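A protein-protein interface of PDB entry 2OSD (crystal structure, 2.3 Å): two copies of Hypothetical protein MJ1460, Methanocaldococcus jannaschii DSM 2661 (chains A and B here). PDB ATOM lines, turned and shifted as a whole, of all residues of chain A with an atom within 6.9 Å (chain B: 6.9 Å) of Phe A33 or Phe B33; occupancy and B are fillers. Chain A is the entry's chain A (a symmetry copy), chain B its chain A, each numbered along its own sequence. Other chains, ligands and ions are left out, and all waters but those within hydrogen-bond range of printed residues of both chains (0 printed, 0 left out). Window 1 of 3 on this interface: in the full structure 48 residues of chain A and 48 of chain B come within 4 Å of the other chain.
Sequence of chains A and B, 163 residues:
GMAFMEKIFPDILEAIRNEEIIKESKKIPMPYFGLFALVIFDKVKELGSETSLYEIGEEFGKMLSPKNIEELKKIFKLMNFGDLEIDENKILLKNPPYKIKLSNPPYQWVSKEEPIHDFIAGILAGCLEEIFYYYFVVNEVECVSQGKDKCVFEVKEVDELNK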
ATOM      1  N   ILE A  12     -12.486 -30.969  -5.639  1.00  0.00           N
ATOM      2  CA  ILE A  12     -13.848 -31.094  -5.133  1.00  0.00           C
ATOM      3  C   ILE A  12     -14.854 -31.488  -6.213  1.00  0.00           C
ATOM      4  O   ILE A  12     -15.776 -32.242  -5.951  1.00  0.00           O
ATOM      5  CB  ILE A  12     -14.293 -29.798  -4.402  1.00  0.00           C
ATOM      6  CG1 ILE A  12     -13.869 -29.874  -2.919  1.00  0.00           C
ATOM      7  CG2 ILE A  12     -15.789 -29.626  -4.481  1.00  0.00           C
ATOM      8  CD1 ILE A  12     -13.557 -28.535  -2.257  1.00  0.00           C
ATOM      9  N   ILE A  28     -18.745 -34.992   8.364  1.00  0.00           N
ATOM     10  CA  ILE A  28     -18.782 -33.860   9.306  1.00  0.00           C
ATOM     11  C   ILE A  28     -20.195 -33.586   9.858  1.00  0.00           C
ATOM     12  O   ILE A  28     -21.165 -33.467   9.093  1.00  0.00           O
ATOM     13  CB  ILE A  28     -18.217 -32.593   8.652  1.00  0.00           C
ATOM     14  CG1 ILE A  28     -18.043 -31.457   9.683  1.00  0.00           C
ATOM     15  CG2 ILE A  28     -19.094 -32.106   7.434  1.00  0.00           C
ATOM     16  CD1 ILE A  28     -17.944 -30.052   8.983  1.00  0.00           C
ATOM     17  N   PRO A  29     -20.320 -33.475  11.187  1.00  0.00           N
ATOM     18  CA  PRO A  29     -21.629 -33.123  11.698  1.00  0.00           C
ATOM     19  C   PRO A  29     -22.260 -31.904  11.070  1.00  0.00           C
ATOM     20  O   PRO A  29     -21.620 -30.888  10.888  1.00  0.00           O
ATOM     21  CB  PRO A  29     -21.391 -32.911  13.141  1.00  0.00           C
ATOM     22  CG  PRO A  29     -20.229 -33.789  13.455  1.00  0.00           C
ATOM     23  CD  PRO A  29     -19.365 -33.736  12.267  1.00  0.00           C
ATOM     24  N   MET A  30     -23.538 -32.012  10.761  1.00  0.00           N
ATOM     25  CA  MET A  30     -24.276 -30.939  10.080  1.00  0.00           C
ATOM     26  C   MET A  30     -24.131 -29.534  10.746  1.00  0.00           C
ATOM     27  O   MET A  30     -23.914 -28.503  10.052  1.00  0.00           O
ATOM     28  CB  MET A  30     -25.751 -31.352  10.024  1.00  0.00           C
ATOM     29  CG  MET A  30     -26.534 -30.704   8.907  1.00  0.00           C
ATOM     30  SD  MET A  30     -25.866 -31.041   7.195  1.00  0.00           S
ATOM     31  CE  MET A  30     -25.417 -32.944   7.342  1.00  0.00           C
ATOM     32  N   PRO A  31     -24.241 -29.467  12.080  1.00  0.00           N
ATOM     33  CA  PRO A  31     -24.040 -28.145  12.711  1.00  0.00           C
ATOM     34  C   PRO A  31     -22.808 -27.357  12.193  1.00  0.00           C
ATOM     35  O   PRO A  31     -22.931 -26.162  11.916  1.00  0.00           O
ATOM     36  CB  PRO A  31     -23.864 -28.496  14.202  1.00  0.00           C
ATOM     37  CG  PRO A  31     -24.682 -29.683  14.385  1.00  0.00           C
ATOM     38  CD  PRO A  31     -24.518 -30.500  13.096  1.00  0.00           C
ATOM     39  N   TYR A  32     -21.653 -28.027  12.048  1.00  0.00           N
ATOM     40  CA  TYR A  32     -20.427 -27.374  11.546  1.00  0.00           C
ATOM     41  C   TYR A  32     -20.555 -26.982  10.096  1.00  0.00           C
ATOM     42  O   TYR A  32     -20.006 -25.977   9.644  1.00  0.00           O
ATOM     43  CB  TYR A  32     -19.242 -28.274  11.718  1.00  0.00           C
ATOM     44  CG  TYR A  32     -18.988 -28.571  13.165  1.00  0.00           C
ATOM     45  CD1 TYR A  32     -18.604 -27.565  14.064  1.00  0.00           C
ATOM     46  CD2 TYR A  32     -19.116 -29.859  13.642  1.00  0.00           C
ATOM     47  CE1 TYR A  32     -18.396 -27.846  15.396  1.00  0.00           C
ATOM     48  CE2 TYR A  32     -18.867 -30.169  14.986  1.00  0.00           C
ATOM     49  CZ  TYR A  32     -18.522 -29.173  15.853  1.00  0.00           C
ATOM     50  OH  TYR A  32     -18.319 -29.515  17.170  1.00  0.00           O
ATOM     51  N   PHE A  33     -21.280 -27.802   9.367  1.00  0.00           N
ATOM     52  CA  PHE A  33     -21.598 -27.505   7.996  1.00  0.00           C
ATOM     53  C   PHE A  33     -22.368 -26.201   7.967  1.00  0.00           C
ATOM     54  O   PHE A  33     -22.043 -25.328   7.196  1.00  0.00           O
ATOM     55  CB  PHE A  33     -22.369 -28.681   7.357  1.00  0.00           C
ATOM     56  CG  PHE A  33     -22.712 -28.484   5.901  1.00  0.00           C
ATOM     57  CD1 PHE A  33     -23.761 -27.691   5.534  1.00  0.00           C
ATOM     58  CD2 PHE A  33     -22.025 -29.145   4.923  1.00  0.00           C
ATOM     59  CE1 PHE A  33     -24.088 -27.502   4.221  1.00  0.00           C
ATOM     60  CE2 PHE A  33     -22.361 -28.976   3.613  1.00  0.00           C
ATOM     61  CZ  PHE A  33     -23.390 -28.142   3.262  1.00  0.00           C
ATOM     62  N   GLY A  34     -23.371 -26.066   8.829  1.00  0.00           N
ATOM     63  CA  GLY A  34     -24.210 -24.848   8.887  1.00  0.00           C
ATOM     64  C   GLY A  34     -23.514 -23.624   9.470  1.00  0.00           C
ATOM     65  O   GLY A  34     -23.828 -22.481   9.113  1.00  0.00           O
ATOM     66  N   LEU A  35     -22.560 -23.857  10.369  1.00  0.00           N
ATOM     67  CA  LEU A  35     -21.657 -22.781  10.810  1.00  0.00           C
ATOM     68  C   LEU A  35     -20.853 -22.192   9.669  1.00  0.00           C
ATOM     69  O   LEU A  35     -20.611 -20.986   9.652  1.00  0.00           O
ATOM     70  CB  LEU A  35     -20.698 -23.275  11.908  1.00  0.00           C
ATOM     71  CG  LEU A  35     -19.855 -22.248  12.636  1.00  0.00           C
ATOM     72  CD1 LEU A  35     -20.778 -21.194  13.319  1.00  0.00           C
ATOM     73  CD2 LEU A  35     -18.912 -22.945  13.669  1.00  0.00           C
ATOM     74  N   PHE A  36     -20.409 -23.019   8.724  1.00  0.00           N
ATOM     75  CA  PHE A  36     -19.626 -22.499   7.599  1.00  0.00           C
ATOM     76  C   PHE A  36     -20.428 -21.481   6.833  1.00  0.00           C
ATOM     77  O   PHE A  36     -19.925 -20.383   6.533  1.00  0.00           O
ATOM     78  CB  PHE A  36     -19.184 -23.595   6.644  1.00  0.00           C
ATOM     79  CG  PHE A  36     -18.232 -23.115   5.560  1.00  0.00           C
ATOM     80  CD1 PHE A  36     -18.684 -22.293   4.502  1.00  0.00           C
ATOM     81  CD2 PHE A  36     -16.891 -23.486   5.592  1.00  0.00           C
ATOM     82  CE1 PHE A  36     -17.789 -21.824   3.497  1.00  0.00           C
ATOM     83  CE2 PHE A  36     -16.010 -23.072   4.601  1.00  0.00           C
ATOM     84  CZ  PHE A  36     -16.456 -22.235   3.544  1.00  0.00           C
ATOM     85  N   ALA A  37     -21.676 -21.812   6.532  1.00  0.00           N
ATOM     86  CA  ALA A  37     -22.518 -20.904   5.769  1.00  0.00           C
ATOM     87  C   ALA A  37     -22.723 -19.645   6.539  1.00  0.00           C
ATOM     88  O   ALA A  37     -22.649 -18.564   5.957  1.00  0.00           O
ATOM     89  CB  ALA A  37     -23.841 -21.521   5.470  1.00  0.00           C
ATOM     90  N   LEU A  38     -23.004 -19.763   7.839  1.00  0.00           N
ATOM     91  CA  LEU A  38     -23.263 -18.594   8.668  1.00  0.00           C
ATOM     92  C   LEU A  38     -22.074 -17.622   8.675  1.00  0.00           C
ATOM     93  O   LEU A  38     -22.266 -16.399   8.605  1.00  0.00           O
ATOM     94  CB  LEU A  38     -23.593 -19.026  10.104  1.00  0.00           C
ATOM     95  CG  LEU A  38     -23.903 -18.015  11.218  1.00  0.00           C
ATOM     96  CD1 LEU A  38     -24.435 -18.809  12.410  1.00  0.00           C
ATOM     97  CD2 LEU A  38     -22.740 -17.058  11.671  1.00  0.00           C
ATOM     98  N   PHE A  60     -25.653 -25.444  -6.238  1.00  0.00           N
ATOM     99  CA  PHE A  60     -25.146 -26.695  -5.663  1.00  0.00           C
ATOM    100  C   PHE A  60     -25.792 -27.886  -6.386  1.00  0.00           C
ATOM    101  O   PHE A  60     -25.098 -28.826  -6.761  1.00  0.00           O
ATOM    102  CB  PHE A  60     -25.523 -26.685  -4.197  1.00  0.00           C
ATOM    103  CG  PHE A  60     -24.785 -27.678  -3.317  1.00  0.00           C
ATOM    104  CD1 PHE A  60     -25.271 -28.959  -3.149  1.00  0.00           C
ATOM    105  CD2 PHE A  60     -23.694 -27.279  -2.560  1.00  0.00           C
ATOM    106  CE1 PHE A  60     -24.619 -29.860  -2.297  1.00  0.00           C
ATOM    107  CE2 PHE A  60     -23.072 -28.150  -1.679  1.00  0.00           C
ATOM    108  CZ  PHE A  60     -23.526 -29.438  -1.554  1.00  0.00           C
ATOM    109  N   MET A  79     -25.321 -37.885   0.679  1.00  0.00           N
ATOM    110  CA  MET A  79     -25.101 -36.610   1.406  1.00  0.00           C
ATOM    111  C   MET A  79     -25.611 -36.668   2.807  1.00  0.00           C
ATOM    112  O   MET A  79     -25.214 -35.871   3.647  1.00  0.00           O
ATOM    113  CB  MET A  79     -25.876 -35.484   0.749  1.00  0.00           C
ATOM    114  CG  MET A  79     -25.428 -35.167  -0.593  1.00  0.00           C
ATOM    115  SD  MET A  79     -26.171 -33.467  -1.188  1.00  0.00           S
ATOM    116  CE  MET A  79     -25.638 -32.378   0.325  1.00  0.00           C
ATOM    117  N   PHE A  81     -28.947 -36.344   3.629  1.00  0.00           N
ATOM    118  CA  PHE A  81     -29.977 -35.343   3.681  1.00  0.00           C
ATOM    119  C   PHE A  81     -31.357 -35.978   3.720  1.00  0.00           C
ATOM    120  O   PHE A  81     -32.377 -35.269   3.674  1.00  0.00           O
ATOM    121  CB  PHE A  81     -29.852 -34.461   2.440  1.00  0.00           C
ATOM    122  CG  PHE A  81     -28.906 -33.339   2.599  1.00  0.00           C
ATOM    123  CD1 PHE A  81     -27.803 -33.447   3.413  1.00  0.00           C
ATOM    124  CD2 PHE A  81     -29.084 -32.189   1.888  1.00  0.00           C
ATOM    125  CE1 PHE A  81     -26.940 -32.424   3.541  1.00  0.00           C
ATOM    126  CE2 PHE A  81     -28.205 -31.149   2.022  1.00  0.00           C
ATOM    127  CZ  PHE A  81     -27.135 -31.276   2.859  1.00  0.00           C
ATOM    128  N   TYR A 107     -31.173 -31.148  10.474  1.00  0.00           N
ATOM    129  CA  TYR A 107     -31.771 -30.221  11.453  1.00  0.00           C
ATOM    130  C   TYR A 107     -33.118 -30.660  12.016  1.00  0.00           C
ATOM    131  O   TYR A 107     -33.952 -29.842  12.310  1.00  0.00           O
ATOM    132  CB  TYR A 107     -31.900 -28.822  10.867  1.00  0.00           C
ATOM    133  CG  TYR A 107     -30.622 -28.277  10.306  1.00  0.00           C
ATOM    134  CD1 TYR A 107     -29.511 -28.098  11.122  1.00  0.00           C
ATOM    135  CD2 TYR A 107     -30.524 -27.924   8.962  1.00  0.00           C
ATOM    136  CE1 TYR A 107     -28.320 -27.607  10.610  1.00  0.00           C
ATOM    137  CE2 TYR A 107     -29.352 -27.408   8.441  1.00  0.00           C
ATOM    138  CZ  TYR A 107     -28.257 -27.241   9.278  1.00  0.00           C
ATOM    139  OH  TYR A 107     -27.081 -26.736   8.783  1.00  0.00           O
ATOM    140  N   PHE A 119     -32.118 -24.156   1.601  1.00  0.00           N
ATOM    141  CA  PHE A 119     -30.983 -24.610   0.846  1.00  0.00           C
ATOM    142  C   PHE A 119     -31.322 -25.883   0.088  1.00  0.00           C
ATOM    143  O   PHE A 119     -31.127 -25.936  -1.112  1.00  0.00           O
ATOM    144  CB  PHE A 119     -29.776 -24.783   1.785  1.00  0.00           C
ATOM    145  CG  PHE A 119     -28.600 -25.440   1.155  1.00  0.00           C
ATOM    146  CD1 PHE A 119     -27.946 -24.849   0.113  1.00  0.00           C
ATOM    147  CD2 PHE A 119     -28.126 -26.638   1.628  1.00  0.00           C
ATOM    148  CE1 PHE A 119     -26.862 -25.457  -0.468  1.00  0.00           C
ATOM    149  CE2 PHE A 119     -27.046 -27.238   1.032  1.00  0.00           C
ATOM    150  CZ  PHE A 119     -26.419 -26.640   0.006  1.00  0.00           C
ATOM    151  N   ILE B  12     -27.975 -22.559  14.848  1.00  0.00           N
ATOM    152  CA  ILE B  12     -26.632 -23.064  14.586  1.00  0.00           C
ATOM    153  C   ILE B  12     -25.627 -22.681  15.670  1.00  0.00           C
ATOM    154  O   ILE B  12     -24.751 -23.463  16.003  1.00  0.00           O
ATOM    155  CB  ILE B  12     -26.134 -22.624  13.182  1.00  0.00           C
ATOM    156  CG1 ILE B  12     -26.592 -23.656  12.128  1.00  0.00           C
ATOM    157  CG2 ILE B  12     -24.630 -22.524  13.156  1.00  0.00           C
ATOM    158  CD1 ILE B  12     -26.846 -23.097  10.731  1.00  0.00           C
ATOM    159  N   ILE B  28     -22.227 -35.285   7.334  1.00  0.00           N
ATOM    160  CA  ILE B  28     -22.149 -35.086   5.876  1.00  0.00           C
ATOM    161  C   ILE B  28     -20.735 -35.330   5.313  1.00  0.00           C
ATOM    162  O   ILE B  28     -19.745 -34.779   5.818  1.00  0.00           O
ATOM    163  CB  ILE B  28     -22.632 -33.682   5.496  1.00  0.00           C
ATOM    164  CG1 ILE B  28     -22.767 -33.528   3.965  1.00  0.00           C
ATOM    165  CG2 ILE B  28     -21.706 -32.549   6.086  1.00  0.00           C
ATOM    166  CD1 ILE B  28     -22.777 -32.016   3.534  1.00  0.00           C
ATOM    167  N   PRO B  29     -20.631 -36.151   4.258  1.00  0.00           N
ATOM    168  CA  PRO B  29     -19.316 -36.304   3.671  1.00  0.00           C
ATOM    169  C   PRO B  29     -18.609 -35.015   3.327  1.00  0.00           C
ATOM    170  O   PRO B  29     -19.191 -34.109   2.765  1.00  0.00           O
ATOM    171  CB  PRO B  29     -19.573 -37.106   2.456  1.00  0.00           C
ATOM    172  CG  PRO B  29     -20.785 -37.904   2.792  1.00  0.00           C
ATOM    173  CD  PRO B  29     -21.621 -37.019   3.616  1.00  0.00           C
ATOM    174  N   MET B  30     -17.333 -34.955   3.655  1.00  0.00           N
ATOM    175  CA  MET B  30     -16.525 -33.744   3.450  1.00  0.00           C
ATOM    176  C   MET B  30     -16.608 -33.148   2.009  1.00  0.00           C
ATOM    177  O   MET B  30     -16.757 -31.909   1.823  1.00  0.00           O
ATOM    178  CB  MET B  30     -15.073 -34.089   3.801  1.00  0.00           C
ATOM    179  CG  MET B  30     -14.234 -32.901   4.206  1.00  0.00           C
ATOM    180  SD  MET B  30     -14.884 -31.961   5.684  1.00  0.00           S
ATOM    181  CE  MET B  30     -15.436 -33.439   6.848  1.00  0.00           C
ATOM    182  N   PRO B  31     -16.523 -34.003   0.981  1.00  0.00           N
ATOM    183  CA  PRO B  31     -16.667 -33.442  -0.380  1.00  0.00           C
ATOM    184  C   PRO B  31     -17.844 -32.447  -0.553  1.00  0.00           C
ATOM    185  O   PRO B  31     -17.652 -31.386  -1.150  1.00  0.00           O
ATOM    186  CB  PRO B  31     -16.891 -34.696  -1.249  1.00  0.00           C
ATOM    187  CG  PRO B  31     -16.141 -35.738  -0.569  1.00  0.00           C
ATOM    188  CD  PRO B  31     -16.322 -35.463   0.930  1.00  0.00           C
ATOM    189  N   TYR B  32     -19.030 -32.782  -0.019  1.00  0.00           N
ATOM    190  CA  TYR B  32     -20.209 -31.898  -0.112  1.00  0.00           C
ATOM    191  C   TYR B  32     -20.031 -30.639   0.698  1.00  0.00           C
ATOM    192  O   TYR B  32     -20.517 -29.565   0.344  1.00  0.00           O
ATOM    193  CB  TYR B  32     -21.443 -32.614   0.343  1.00  0.00           C
ATOM    194  CG  TYR B  32     -21.742 -33.794  -0.532  1.00  0.00           C
ATOM    195  CD1 TYR B  32     -22.090 -33.638  -1.882  1.00  0.00           C
ATOM    196  CD2 TYR B  32     -21.692 -35.072  -0.016  1.00  0.00           C
ATOM    197  CE1 TYR B  32     -22.341 -34.730  -2.681  1.00  0.00           C
ATOM    198  CE2 TYR B  32     -21.985 -36.192  -0.805  1.00  0.00           C
ATOM    199  CZ  TYR B  32     -22.295 -36.023  -2.124  1.00  0.00           C
ATOM    200  OH  TYR B  32     -22.543 -37.151  -2.871  1.00  0.00           O
ATOM    201  N   PHE B  33     -19.336 -30.791   1.804  1.00  0.00           N
ATOM    202  CA  PHE B  33     -18.974 -29.666   2.624  1.00  0.00           C
ATOM    203  C   PHE B  33     -18.136 -28.726   1.783  1.00  0.00           C
ATOM    204  O   PHE B  33     -18.398 -27.546   1.759  1.00  0.00           O
ATOM    205  CB  PHE B  33     -18.253 -30.144   3.904  1.00  0.00           C
ATOM    206  CG  PHE B  33     -17.870 -29.037   4.855  1.00  0.00           C
ATOM    207  CD1 PHE B  33     -16.773 -28.260   4.614  1.00  0.00           C
ATOM    208  CD2 PHE B  33     -18.571 -28.829   6.008  1.00  0.00           C
ATOM    209  CE1 PHE B  33     -16.410 -27.254   5.464  1.00  0.00           C
ATOM    210  CE2 PHE B  33     -18.200 -27.841   6.870  1.00  0.00           C
ATOM    211  CZ  PHE B  33     -17.122 -27.044   6.588  1.00  0.00           C
ATOM    212  N   GLY B  34     -17.145 -29.260   1.076  1.00  0.00           N
ATOM    213  CA  GLY B  34     -16.244 -28.445   0.230  1.00  0.00           C
ATOM    214  C   GLY B  34     -16.886 -27.898  -1.039  1.00  0.00           C
ATOM    215  O   GLY B  34     -16.505 -26.831  -1.538  1.00  0.00           O
ATOM    216  N   LEU B  35     -17.869 -28.624  -1.566  1.00  0.00           N
ATOM    217  CA  LEU B  35     -18.723 -28.080  -2.635  1.00  0.00           C
ATOM    218  C   LEU B  35     -19.471 -26.835  -2.204  1.00  0.00           C
ATOM    219  O   LEU B  35     -19.648 -25.921  -3.009  1.00  0.00           O
ATOM    220  CB  LEU B  35     -19.729 -29.132  -3.134  1.00  0.00           C
ATOM    221  CG  LEU B  35     -20.531 -28.820  -4.381  1.00  0.00           C
ATOM    222  CD1 LEU B  35     -19.568 -28.552  -5.576  1.00  0.00           C
ATOM    223  CD2 LEU B  35     -21.531 -29.980  -4.694  1.00  0.00           C
ATOM    224  N   PHE B  36     -19.939 -26.785  -0.959  1.00  0.00           N
ATOM    225  CA  PHE B  36     -20.669 -25.603  -0.493  1.00  0.00           C
ATOM    226  C   PHE B  36     -19.800 -24.379  -0.596  1.00  0.00           C
ATOM    227  O   PHE B  36     -20.237 -23.340  -1.124  1.00  0.00           O
ATOM    228  CB  PHE B  36     -21.149 -25.745   0.941  1.00  0.00           C
ATOM    229  CG  PHE B  36     -22.052 -24.610   1.400  1.00  0.00           C
ATOM    230  CD1 PHE B  36     -21.536 -23.316   1.638  1.00  0.00           C
ATOM    231  CD2 PHE B  36     -23.411 -24.835   1.599  1.00  0.00           C
ATOM    232  CE1 PHE B  36     -22.383 -22.246   2.047  1.00  0.00           C
ATOM    233  CE2 PHE B  36     -24.248 -23.816   2.035  1.00  0.00           C
ATOM    234  CZ  PHE B  36     -23.737 -22.510   2.262  1.00  0.00           C
ATOM    235  N   ALA B  37     -18.564 -24.486  -0.124  1.00  0.00           N
ATOM    236  CA  ALA B  37     -17.660 -23.348  -0.155  1.00  0.00           C
ATOM    237  C   ALA B  37     -17.404 -22.948  -1.567  1.00  0.00           C
ATOM    238  O   ALA B  37     -17.409 -21.755  -1.866  1.00  0.00           O
ATOM    239  CB  ALA B  37     -16.366 -23.671   0.508  1.00  0.00           C
ATOM    240  N   LEU B  38     -17.157 -23.925  -2.443  1.00  0.00           N
ATOM    241  CA  LEU B  38     -16.854 -23.634  -3.838  1.00  0.00           C
ATOM    242  C   LEU B  38     -17.989 -22.859  -4.521  1.00  0.00           C
ATOM    243  O   LEU B  38     -17.732 -21.921  -5.289  1.00  0.00           O
ATOM    244  CB  LEU B  38     -16.576 -24.938  -4.601  1.00  0.00           C
ATOM    245  CG  LEU B  38     -16.236 -24.958  -6.099  1.00  0.00           C
ATOM    246  CD1 LEU B  38     -15.771 -26.374  -6.434  1.00  0.00           C
ATOM    247  CD2 LEU B  38     -17.356 -24.495  -7.102  1.00  0.00           C
ATOM    248  N   PHE B  60     -14.525 -18.778  11.841  1.00  0.00           N
ATOM    249  CA  PHE B  60     -15.109 -20.061  12.248  1.00  0.00           C
ATOM    250  C   PHE B  60     -14.512 -20.487  13.598  1.00  0.00           C
ATOM    251  O   PHE B  60     -15.247 -20.891  14.492  1.00  0.00           O
ATOM    252  CB  PHE B  60     -14.762 -21.061  11.165  1.00  0.00           C
ATOM    253  CG  PHE B  60     -15.569 -22.346  11.168  1.00  0.00           C
ATOM    254  CD1 PHE B  60     -15.155 -23.430  11.917  1.00  0.00           C
ATOM    255  CD2 PHE B  60     -16.653 -22.504  10.317  1.00  0.00           C
ATOM    256  CE1 PHE B  60     -15.871 -24.634  11.879  1.00  0.00           C
ATOM    257  CE2 PHE B  60     -17.338 -23.707  10.241  1.00  0.00           C
ATOM    258  CZ  PHE B  60     -16.956 -24.765  11.024  1.00  0.00           C
ATOM    259  N   MET B  79     -15.656 -32.593  15.096  1.00  0.00           N
ATOM    260  CA  MET B  79     -15.823 -32.131  13.697  1.00  0.00           C
ATOM    261  C   MET B  79     -15.346 -33.143  12.711  1.00  0.00           C
ATOM    262  O   MET B  79     -15.717 -33.100  11.544  1.00  0.00           O
ATOM    263  CB  MET B  79     -14.977 -30.898  13.440  1.00  0.00           C
ATOM    264  CG  MET B  79     -15.380 -29.738  14.210  1.00  0.00           C
ATOM    265  SD  MET B  79     -14.536 -28.123  13.520  1.00  0.00           S
ATOM    266  CE  MET B  79     -15.041 -28.311  11.658  1.00  0.00           C
ATOM    267  N   PHE B  81     -12.015 -33.634  11.953  1.00  0.00           N
ATOM    268  CA  PHE B  81     -10.935 -32.986  11.262  1.00  0.00           C
ATOM    269  C   PHE B  81      -9.591 -33.554  11.689  1.00  0.00           C
ATOM    270  O   PHE B  81      -8.534 -33.053  11.267  1.00  0.00           O
ATOM    271  CB  PHE B  81     -10.987 -31.494  11.583  1.00  0.00           C
ATOM    272  CG  PHE B  81     -11.876 -30.723  10.691  1.00  0.00           C
ATOM    273  CD1 PHE B  81     -12.999 -31.292  10.139  1.00  0.00           C
ATOM    274  CD2 PHE B  81     -11.623 -29.406  10.446  1.00  0.00           C
ATOM    275  CE1 PHE B  81     -13.810 -30.578   9.338  1.00  0.00           C
ATOM    276  CE2 PHE B  81     -12.448 -28.682   9.629  1.00  0.00           C
ATOM    277  CZ  PHE B  81     -13.540 -29.283   9.073  1.00  0.00           C
ATOM    278  N   TYR B 107      -9.659 -34.529   3.441  1.00  0.00           N
ATOM    279  CA  TYR B 107      -9.032 -34.536   2.106  1.00  0.00           C
ATOM    280  C   TYR B 107      -7.722 -35.310   2.013  1.00  0.00           C
ATOM    281  O   TYR B 107      -6.853 -34.948   1.262  1.00  0.00           O
ATOM    282  CB  TYR B 107      -8.817 -33.115   1.600  1.00  0.00           C
ATOM    283  CG  TYR B 107     -10.052 -32.268   1.622  1.00  0.00           C
ATOM    284  CD1 TYR B 107     -11.169 -32.627   0.875  1.00  0.00           C
ATOM    285  CD2 TYR B 107     -10.104 -31.098   2.375  1.00  0.00           C
ATOM    286  CE1 TYR B 107     -12.322 -31.857   0.898  1.00  0.00           C
ATOM    287  CE2 TYR B 107     -11.237 -30.305   2.389  1.00  0.00           C
ATOM    288  CZ  TYR B 107     -12.338 -30.687   1.636  1.00  0.00           C
ATOM    289  OH  TYR B 107     -13.475 -29.919   1.637  1.00  0.00           O
ATOM    290  N   PHE B 119      -8.163 -23.449   5.312  1.00  0.00           N
ATOM    291  CA  PHE B 119      -9.305 -23.215   6.153  1.00  0.00           C
ATOM    292  C   PHE B 119      -9.017 -23.661   7.576  1.00  0.00           C
ATOM    293  O   PHE B 119      -9.190 -22.882   8.495  1.00  0.00           O
ATOM    294  CB  PHE B 119     -10.538 -23.910   5.550  1.00  0.00           C
ATOM    295  CG  PHE B 119     -11.733 -23.909   6.434  1.00  0.00           C
ATOM    296  CD1 PHE B 119     -12.334 -22.736   6.793  1.00  0.00           C
ATOM    297  CD2 PHE B 119     -12.280 -25.085   6.881  1.00  0.00           C
ATOM    298  CE1 PHE B 119     -13.436 -22.737   7.610  1.00  0.00           C
ATOM    299  CE2 PHE B 119     -13.378 -25.069   7.704  1.00  0.00           C
ATOM    300  CZ  PHE B 119     -13.951 -23.904   8.047  1.00  0.00           C
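N of Ile B28 is in hydrogen-bond range of O of Ile A28 (2.7 Å).
CG2 of Ile A12 touches CD1 of Leu B38, 3.8 Å away. O of Met B79 touches CG1 of Ile A28, at 3.4 Å. Met A30 touches Ile B28. CG of Met B79 touches CZ of Tyr A32, at 3.6 Å. Phe A33 touches Phe B33 (CE2 to CA, 3.6 Å). Phe A33 touches Phe B36. Gly A34 touches Ile B12. Phe A60 touches Leu B35 (CZ to CD2, 3.8 Å). Phe B36 touches Phe A60. Phe B36 touches Phe A119 (CD2 to CZ, 3.9 Å).
Of the printed residues of chain B, Pro A29 touches Met B79. Printed residues of chain B within 4 Å of Phe A33: Ile B28, Tyr B32, Phe B33 and Phe B36. Printed residues of chain A within 4 Å of Ile B28: Ile A28, Met A30, Phe A33 and Met A79. Of chain A, only Ile A28 (3.1 Å), Tyr A32 (3.8 Å), Phe A33 (3.6 Å) and Phe A36 (3.7 Å) come within 4 Å of Phe B33. Printed residues of chain A within 4 Å of Phe B60: Tyr A32 (3.6 Å), Leu A35 (3.8 Å) and Phe A36 (3.5 Å). Of the printed residues of chain A, Phe B119 touches Phe A36 (3.9 Å). The nearest residue of chain A that does not touch Phe B33 is Phe A60 (5.5 Å).
Printed residues of chain A that touch a printed residue of chain B: Ile A12, Ile A28, Pro A29, Met A30, Tyr A32, Phe A33, Gly A34, Leu A35, Phe A36, Ala A37, Leu A38, Phe A60, Met A79 and Phe A119. Of the 17 printed residues of chain B, 14 touch a printed residue of chain A. Hydrophobic or aromatic side chains of chain B within 4 Å of the printed part of chain A: Ile B12, Ile B28, Pro B29, Met B30, Tyr B32, Phe B33, Leu B35, Phe B36, Ala B37, Leu B38, Phe B60, Met B79 and Phe B119. Among the printed residues, 32 pairs touch across the chains. Among the printed residues, no Asp or Glu carboxylate lies within 4 Å of a Lys or Arg side-chain nitrogen of the other chain.
Ile A28 touches Met B30, and with the chains exchanged Met A30 touches Ile B28. Tyr A32 touches Phe B60, and with the chains exchanged Phe A60 touches Tyr B32. Phe A33 touches Phe B36, and with the chains exchanged Phe A36 touches Phe B33. Phe A36 touches Phe B119, and with the chains exchanged Phe A119 touches Phe B36. Positions printed for both chains: 12, 28, 29, 30, 31, 32, 33, 34, 35, 36, 37, 38, 60, 79, 81, 107 and 119. Of the 32 pairs that touch across the chains among the printed residues, 32 have their exchanged pair printed and touching as well.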
